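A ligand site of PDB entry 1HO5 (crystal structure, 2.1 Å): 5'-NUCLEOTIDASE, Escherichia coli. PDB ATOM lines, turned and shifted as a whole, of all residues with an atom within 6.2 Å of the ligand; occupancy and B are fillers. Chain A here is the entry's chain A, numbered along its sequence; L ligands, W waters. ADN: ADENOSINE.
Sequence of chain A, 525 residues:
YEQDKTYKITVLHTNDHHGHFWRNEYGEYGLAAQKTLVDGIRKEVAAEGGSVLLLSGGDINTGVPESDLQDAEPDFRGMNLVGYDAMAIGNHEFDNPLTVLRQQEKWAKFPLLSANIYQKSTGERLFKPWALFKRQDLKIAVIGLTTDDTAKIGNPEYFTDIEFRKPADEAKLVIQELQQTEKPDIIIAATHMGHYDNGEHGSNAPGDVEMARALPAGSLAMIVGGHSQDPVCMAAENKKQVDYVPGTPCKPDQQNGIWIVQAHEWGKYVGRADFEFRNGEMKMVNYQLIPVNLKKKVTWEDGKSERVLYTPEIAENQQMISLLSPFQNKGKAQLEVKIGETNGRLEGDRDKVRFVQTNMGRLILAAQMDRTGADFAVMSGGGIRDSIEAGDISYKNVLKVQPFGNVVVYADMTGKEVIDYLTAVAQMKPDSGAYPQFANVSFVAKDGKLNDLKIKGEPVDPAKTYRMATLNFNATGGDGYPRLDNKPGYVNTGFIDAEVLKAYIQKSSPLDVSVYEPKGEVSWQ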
ATOM      1  N   ASN A  91      25.779  -6.673 -13.823  1.00  0.00           N
ATOM      2  CA  ASN A  91      25.337  -5.283 -13.601  1.00  0.00           C
ATOM      3  C   ASN A  91      23.967  -4.986 -14.201  1.00  0.00           C
ATOM      4  O   ASN A  91      23.186  -4.238 -13.600  1.00  0.00           O
ATOM      5  CB  ASN A  91      26.364  -4.277 -14.117  1.00  0.00           C
ATOM      6  CG  ASN A  91      26.720  -4.490 -15.570  1.00  0.00           C
ATOM      7  OD1 ASN A  91      27.128  -5.601 -15.983  1.00  0.00           O
ATOM      8  ND2 ASN A  91      26.610  -3.431 -16.353  1.00  0.00           N
ATOM      9  N   HIS A  92      23.674  -5.537 -15.374  1.00  0.00           N
ATOM     10  CA  HIS A  92      22.356  -5.258 -15.942  1.00  0.00           C
ATOM     11  C   HIS A  92      21.216  -5.874 -15.148  1.00  0.00           C
ATOM     12  O   HIS A  92      20.086  -5.631 -15.475  1.00  0.00           O
ATOM     13  CB  HIS A  92      22.262  -5.672 -17.403  1.00  0.00           C
ATOM     14  CG  HIS A  92      22.974  -4.726 -18.295  1.00  0.00           C
ATOM     15  ND1 HIS A  92      22.373  -3.600 -18.794  1.00  0.00           N
ATOM     16  CD2 HIS A  92      24.280  -4.650 -18.647  1.00  0.00           C
ATOM     17  CE1 HIS A  92      23.273  -2.864 -19.416  1.00  0.00           C
ATOM     18  NE2 HIS A  92      24.443  -3.481 -19.334  1.00  0.00           N
ATOM     19  N   PHE A  94      20.573  -4.889 -12.576  1.00  0.00           N
ATOM     20  CA  PHE A  94      20.185  -3.708 -11.784  1.00  0.00           C
ATOM     21  C   PHE A  94      19.620  -2.630 -12.675  1.00  0.00           C
ATOM     22  O   PHE A  94      19.592  -1.444 -12.308  1.00  0.00           O
ATOM     23  CB  PHE A  94      21.396  -3.167 -10.979  1.00  0.00           C
ATOM     24  CG  PHE A  94      21.750  -4.034  -9.813  1.00  0.00           C
ATOM     25  CD1 PHE A  94      21.037  -3.934  -8.633  1.00  0.00           C
ATOM     26  CD2 PHE A  94      22.767  -5.011  -9.919  1.00  0.00           C
ATOM     27  CE1 PHE A  94      21.300  -4.776  -7.554  1.00  0.00           C
ATOM     28  CE2 PHE A  94      23.044  -5.867  -8.861  1.00  0.00           C
ATOM     29  CZ  PHE A  94      22.315  -5.754  -7.669  1.00  0.00           C
ATOM     30  N   ASP A  95      19.184  -3.054 -13.856  1.00  0.00           N
ATOM     31  CA  ASP A  95      18.559  -2.153 -14.840  1.00  0.00           C
ATOM     32  C   ASP A  95      17.130  -1.833 -14.401  1.00  0.00           C
ATOM     33  O   ASP A  95      16.545  -0.818 -14.797  1.00  0.00           O
ATOM     34  CB  ASP A  95      18.514  -2.808 -16.217  1.00  0.00           C
ATOM     35  CG  ASP A  95      19.809  -2.645 -16.989  1.00  0.00           C
ATOM     36  OD1 ASP A  95      20.773  -2.125 -16.411  1.00  0.00           O
ATOM     37  OD2 ASP A  95      19.865  -3.037 -18.183  1.00  0.00           O
ATOM     38  N   ILE A 153      28.401   2.957 -13.302  1.00  0.00           N
ATOM     39  CA  ILE A 153      27.867   3.195 -14.619  1.00  0.00           C
ATOM     40  C   ILE A 153      26.346   3.026 -14.700  1.00  0.00           C
ATOM     41  O   ILE A 153      25.735   3.298 -15.738  1.00  0.00           O
ATOM     42  CB  ILE A 153      28.552   2.296 -15.684  1.00  0.00           C
ATOM     43  CG1 ILE A 153      28.337   0.823 -15.381  1.00  0.00           C
ATOM     44  CG2 ILE A 153      30.062   2.604 -15.729  1.00  0.00           C
ATOM     45  CD1 ILE A 153      29.196  -0.073 -16.225  1.00  0.00           C
ATOM     46  N   GLY A 154      25.725   2.621 -13.596  1.00  0.00           N
ATOM     47  CA  GLY A 154      24.300   2.409 -13.612  1.00  0.00           C
ATOM     48  C   GLY A 154      23.438   3.562 -13.085  1.00  0.00           C
ATOM     49  O   GLY A 154      23.934   4.651 -12.761  1.00  0.00           O
ATOM     50  N   ASN A 155      22.128   3.318 -13.030  1.00  0.00           N
ATOM     51  CA  ASN A 155      21.181   4.313 -12.551  1.00  0.00           C
ATOM     52  C   ASN A 155      21.446   4.659 -11.069  1.00  0.00           C
ATOM     53  O   ASN A 155      21.253   3.828 -10.178  1.00  0.00           O
ATOM     54  CB  ASN A 155      19.746   3.798 -12.755  1.00  0.00           C
ATOM     55  CG  ASN A 155      18.701   4.758 -12.225  1.00  0.00           C
ATOM     56  OD1 ASN A 155      18.881   5.969 -12.296  1.00  0.00           O
ATOM     57  ND2 ASN A 155      17.599   4.214 -11.717  1.00  0.00           N
ATOM     58  N   TYR A 158      19.105   3.581  -7.948  1.00  0.00           N
ATOM     59  CA  TYR A 158      19.024   2.206  -7.471  1.00  0.00           C
ATOM     60  C   TYR A 158      20.027   1.851  -6.400  1.00  0.00           C
ATOM     61  O   TYR A 158      19.796   0.980  -5.572  1.00  0.00           O
ATOM     62  CB  TYR A 158      19.203   1.217  -8.630  1.00  0.00           C
ATOM     63  CG  TYR A 158      18.062   1.251  -9.608  1.00  0.00           C
ATOM     64  CD1 TYR A 158      16.760   1.608  -9.195  1.00  0.00           C
ATOM     65  CD2 TYR A 158      18.265   0.914 -10.955  1.00  0.00           C
ATOM     66  CE1 TYR A 158      15.686   1.630 -10.113  1.00  0.00           C
ATOM     67  CE2 TYR A 158      17.205   0.932 -11.876  1.00  0.00           C
ATOM     68  CZ  TYR A 158      15.919   1.286 -11.445  1.00  0.00           C
ATOM     69  OH  TYR A 158      14.897   1.324 -12.354  1.00  0.00           O
ATOM     70  N   ARG A 350      27.876   0.718 -30.754  1.00  0.00           N
ATOM     71  CA  ARG A 350      28.726   1.180 -29.663  1.00  0.00           C
ATOM     72  C   ARG A 350      30.046   1.775 -30.164  1.00  0.00           C
ATOM     73  O   ARG A 350      30.417   2.895 -29.798  1.00  0.00           O
ATOM     74  CB  ARG A 350      29.000   0.030 -28.683  1.00  0.00           C
ATOM     75  CG  ARG A 350      29.220   0.479 -27.248  1.00  0.00           C
ATOM     76  CD  ARG A 350      30.303  -0.335 -26.569  1.00  0.00           C
ATOM     77  NE  ARG A 350      29.809  -1.117 -25.430  1.00  0.00           N
ATOM     78  CZ  ARG A 350      30.601  -1.704 -24.534  1.00  0.00           C
ATOM     79  NH1 ARG A 350      31.920  -1.601 -24.645  1.00  0.00           N
ATOM     80  NH2 ARG A 350      30.077  -2.404 -23.536  1.00  0.00           N
ATOM     81  N   ARG A 354      30.035   5.517 -28.952  1.00  0.00           N
ATOM     82  CA  ARG A 354      30.912   5.567 -27.785  1.00  0.00           C
ATOM     83  C   ARG A 354      32.189   6.378 -28.085  1.00  0.00           C
ATOM     84  O   ARG A 354      32.895   6.818 -27.180  1.00  0.00           O
ATOM     85  CB  ARG A 354      31.286   4.126 -27.371  1.00  0.00           C
ATOM     86  CG  ARG A 354      31.426   3.876 -25.857  1.00  0.00           C
ATOM     87  CD  ARG A 354      30.091   3.992 -25.142  1.00  0.00           C
ATOM     88  NE  ARG A 354      29.269   2.787 -25.164  1.00  0.00           N
ATOM     89  CZ  ARG A 354      29.280   1.837 -24.236  1.00  0.00           C
ATOM     90  NH1 ARG A 354      30.087   1.924 -23.190  1.00  0.00           N
ATOM     91  NH2 ARG A 354      28.433   0.827 -24.303  1.00  0.00           N
ATOM     92  N   SER A 380      24.080   9.964 -23.144  1.00  0.00           N
ATOM     93  CA  SER A 380      25.261   9.104 -23.103  1.00  0.00           C
ATOM     94  C   SER A 380      25.264   8.228 -24.346  1.00  0.00           C
ATOM     95  O   SER A 380      24.231   7.741 -24.780  1.00  0.00           O
ATOM     96  CB  SER A 380      25.253   8.205 -21.857  1.00  0.00           C
ATOM     97  OG  SER A 380      25.325   8.953 -20.653  1.00  0.00           O
ATOM     98  N   GLY A 381      26.431   8.059 -24.956  1.00  0.00           N
ATOM     99  CA  GLY A 381      26.511   7.199 -26.123  1.00  0.00           C
ATOM    100  C   GLY A 381      26.159   5.812 -25.635  1.00  0.00           C
ATOM    101  O   GLY A 381      25.644   4.988 -26.385  1.00  0.00           O
ATOM    102  N   GLY A 382      26.433   5.568 -24.351  1.00  0.00           N
ATOM    103  CA  GLY A 382      26.119   4.286 -23.732  1.00  0.00           C
ATOM    104  C   GLY A 382      24.628   4.109 -23.585  1.00  0.00           C
ATOM    105  O   GLY A 382      24.149   3.127 -23.010  1.00  0.00           O
ATOM    106  N   GLY A 383      23.877   5.085 -24.090  1.00  0.00           N
ATOM    107  CA  GLY A 383      22.439   5.010 -24.028  1.00  0.00           C
ATOM    108  C   GLY A 383      21.904   4.553 -25.373  1.00  0.00           C
ATOM    109  O   GLY A 383      20.742   4.171 -25.481  1.00  0.00           O
ATOM    110  N   ARG A 385      21.721   1.843 -27.718  1.00  0.00           N
ATOM    111  CA  ARG A 385      21.997   0.408 -27.743  1.00  0.00           C
ATOM    112  C   ARG A 385      21.973  -0.223 -29.125  1.00  0.00           C
ATOM    113  O   ARG A 385      22.491  -1.321 -29.315  1.00  0.00           O
ATOM    114  CB  ARG A 385      21.034  -0.301 -26.805  1.00  0.00           C
ATOM    115  CG  ARG A 385      21.008   0.324 -25.403  1.00  0.00           C
ATOM    116  CD  ARG A 385      22.067  -0.221 -24.457  1.00  0.00           C
ATOM    117  NE  ARG A 385      23.398  -0.301 -25.041  1.00  0.00           N
ATOM    118  CZ  ARG A 385      24.466  -0.801 -24.425  1.00  0.00           C
ATOM    119  NH1 ARG A 385      24.358  -1.274 -23.180  1.00  0.00           N
ATOM    120  NH2 ARG A 385      25.640  -0.849 -25.062  1.00  0.00           N
ATOM    121  N   PHE A 404      16.429   0.952 -21.877  1.00  0.00           N
ATOM    122  CA  PHE A 404      16.498   1.170 -20.443  1.00  0.00           C
ATOM    123  C   PHE A 404      15.256   1.741 -19.787  1.00  0.00           C
ATOM    124  O   PHE A 404      15.126   1.691 -18.568  1.00  0.00           O
ATOM    125  CB  PHE A 404      17.689   2.072 -20.150  1.00  0.00           C
ATOM    126  CG  PHE A 404      19.024   1.465 -20.466  1.00  0.00           C
ATOM    127  CD1 PHE A 404      19.520   0.402 -19.695  1.00  0.00           C
ATOM    128  CD2 PHE A 404      19.813   1.957 -21.484  1.00  0.00           C
ATOM    129  CE1 PHE A 404      20.779  -0.126 -19.939  1.00  0.00           C
ATOM    130  CE2 PHE A 404      21.072   1.442 -21.749  1.00  0.00           C
ATOM    131  CZ  PHE A 404      21.562   0.410 -20.978  1.00  0.00           C
ATOM    132  N   ASN A 406      14.454   4.936 -19.826  1.00  0.00           N
ATOM    133  CA  ASN A 406      14.832   6.218 -19.224  1.00  0.00           C
ATOM    134  C   ASN A 406      13.714   7.272 -19.439  1.00  0.00           C
ATOM    135  O   ASN A 406      12.856   7.113 -20.318  1.00  0.00           O
ATOM    136  CB  ASN A 406      16.145   6.723 -19.832  1.00  0.00           C
ATOM    137  CG  ASN A 406      17.389   6.081 -19.201  1.00  0.00           C
ATOM    138  OD1 ASN A 406      18.497   6.295 -19.676  1.00  0.00           O
ATOM    139  ND2 ASN A 406      17.214   5.306 -18.134  1.00  0.00           N
ATOM    140  N   SER A 432      33.861   5.260 -23.836  1.00  0.00           N
ATOM    141  CA  SER A 432      33.158   5.293 -22.573  1.00  0.00           C
ATOM    142  C   SER A 432      31.669   5.471 -22.840  1.00  0.00           C
ATOM    143  O   SER A 432      31.270   6.174 -23.776  1.00  0.00           O
ATOM    144  CB  SER A 432      33.658   6.455 -21.713  1.00  0.00           C
ATOM    145  OG  SER A 432      33.038   6.452 -20.425  1.00  0.00           O
ATOM    146  N   GLY A 433      30.842   4.822 -22.032  1.00  0.00           N
ATOM    147  CA  GLY A 433      29.409   4.958 -22.206  1.00  0.00           C
ATOM    148  C   GLY A 433      29.036   6.378 -21.855  1.00  0.00           C
ATOM    149  O   GLY A 433      28.031   6.904 -22.331  1.00  0.00           O
ATOM    150  N   ALA A 434      29.858   7.000 -21.021  1.00  0.00           N
ATOM    151  CA  ALA A 434      29.634   8.359 -20.573  1.00  0.00           C
ATOM    152  C   ALA A 434      29.992   9.351 -21.686  1.00  0.00           C
ATOM    153  O   ALA A 434      29.772  10.560 -21.558  1.00  0.00           O
ATOM    154  CB  ALA A 434      30.453   8.647 -19.325  1.00  0.00           C
ATOM    155  N   PHE A 473      18.546   9.629 -16.163  1.00  0.00           N
ATOM    156  CA  PHE A 473      19.781   8.910 -15.884  1.00  0.00           C
ATOM    157  C   PHE A 473      20.915   9.939 -15.790  1.00  0.00           C
ATOM    158  O   PHE A 473      21.505  10.146 -14.729  1.00  0.00           O
ATOM    159  CB  PHE A 473      20.077   7.926 -17.025  1.00  0.00           C
ATOM    160  CG  PHE A 473      21.404   7.197 -16.885  1.00  0.00           C
ATOM    161  CD1 PHE A 473      21.550   6.140 -15.987  1.00  0.00           C
ATOM    162  CD2 PHE A 473      22.519   7.612 -17.614  1.00  0.00           C
ATOM    163  CE1 PHE A 473      22.794   5.512 -15.806  1.00  0.00           C
ATOM    164  CE2 PHE A 473      23.762   6.984 -17.443  1.00  0.00           C
ATOM    165  CZ  PHE A 473      23.896   5.931 -16.533  1.00  0.00           C
ATOM    166  N   ASP A 479      26.838   8.057 -15.212  1.00  0.00           N
ATOM    167  CA  ASP A 479      28.095   8.287 -15.929  1.00  0.00           C
ATOM    168  C   ASP A 479      28.799   9.495 -15.303  1.00  0.00           C
ATOM    169  O   ASP A 479      29.668  10.123 -15.915  1.00  0.00           O
ATOM    170  CB  ASP A 479      27.859   8.528 -17.424  1.00  0.00           C
ATOM    171  CG  ASP A 479      27.575   7.249 -18.176  1.00  0.00           C
ATOM    172  OD1 ASP A 479      27.861   6.186 -17.620  1.00  0.00           O
ATOM    173  OD2 ASP A 479      27.074   7.290 -19.316  1.00  0.00           O
HETATM  174  O5' ADN L   1      27.114  -0.104 -20.934  1.00  0.00           O
HETATM  175  C5' ADN L   1      27.275   0.840 -19.888  1.00  0.00           C
HETATM  176  C4' ADN L   1      26.578   2.133 -20.234  1.00  0.00           C
HETATM  177  O4' ADN L   1      25.160   1.856 -20.442  1.00  0.00           O
HETATM  178  C3' ADN L   1      26.583   3.205 -19.144  1.00  0.00           C
HETATM  179  O3' ADN L   1      27.797   3.953 -19.144  1.00  0.00           O
HETATM  180  C2' ADN L   1      25.372   4.047 -19.535  1.00  0.00           C
HETATM  181  O2' ADN L   1      25.696   4.936 -20.586  1.00  0.00           O
HETATM  182  C1' ADN L   1      24.390   2.974 -20.013  1.00  0.00           C
HETATM  183  N9  ADN L   1      23.496   2.523 -18.946  1.00  0.00           N
HETATM  184  C8  ADN L   1      23.690   1.537 -18.020  1.00  0.00           C
HETATM  185  N7  ADN L   1      22.683   1.382 -17.191  1.00  0.00           N
HETATM  186  C5  ADN L   1      21.767   2.330 -17.612  1.00  0.00           C
HETATM  187  C6  ADN L   1      20.489   2.686 -17.143  1.00  0.00           C
HETATM  188  N6  ADN L   1      19.874   2.095 -16.123  1.00  0.00           N
HETATM  189  N1  ADN L   1      19.854   3.698 -17.773  1.00  0.00           N
HETATM  190  C2  ADN L   1      20.473   4.303 -18.794  1.00  0.00           C
HETATM  191  N3  ADN L   1      21.651   4.056 -19.332  1.00  0.00           N
HETATM  192  C4  ADN L   1      22.258   3.039 -18.686  1.00  0.00           C
HETATM  193  O   HOH W   1      21.002   0.581 -13.372  1.00  0.00           O
HETATM  194  O   HOH W   2      22.916  -0.743 -15.373  1.00  0.00           O
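OD1 of Asp 479 is in hydrogen-bond range of O3' of the ligand.
N1 of the ligand sits at hydrogen-bond distance from ND2 of Asn 406 (3.1 Å).
The backbone carbonyl oxygen of Gly 382 sits close to an oxygen (O2') of the ligand, 3.4 Å away.
The side-chain carboxylate of Asp 479 sits at hydrogen-bond distance from the side-chain hydroxyl of Ser 380 (2.8 Å).
The side-chain carboxylate of Asp 479 lies close to the backbone NH of Ala 434.
The backbone NH of Gly 382 lies within hydrogen-bond range of the backbone carbonyl oxygen of Gly 433, at 2.9 Å.
The backbone carbonyl oxygen (O) of Gly 433 sits at hydrogen-bond distance from the backbone NH (N) of Gly 381 (3.3 Å).
The guanidinium group (NH2) of Arg 354 sits close to the guanidinium group (NE) of Arg 350 (2.6 Å).
Residues that only touch the ligand: Phe 473 (3.5 Å), Ile 153 (3.5 Å), Phe 404 (3.5 Å), Gly 433 (3.5 Å), Ser 380 (3.5 Å), Arg 354 (3.7 Å), Arg 385 (3.7 Å), Asn 155 (3.8 Å) and Gly 383 (3.95 Å).
Hydrophobic or aromatic side chains within 4 Å of the ligand: Ile 153, Phe 404 and Phe 473.
Of the 22 residues printed, 12 come within 4 Å of the ligand.
Water W2 lies within hydrogen-bond range of the side-chain carboxylate of Asp 95 (2.8 Å) and a nitrogen (N7) of the ligand (2.8 Å).
Water W1 lies within hydrogen-bond range of O of Phe 94, N of Asn 155 and N6 of the ligand.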
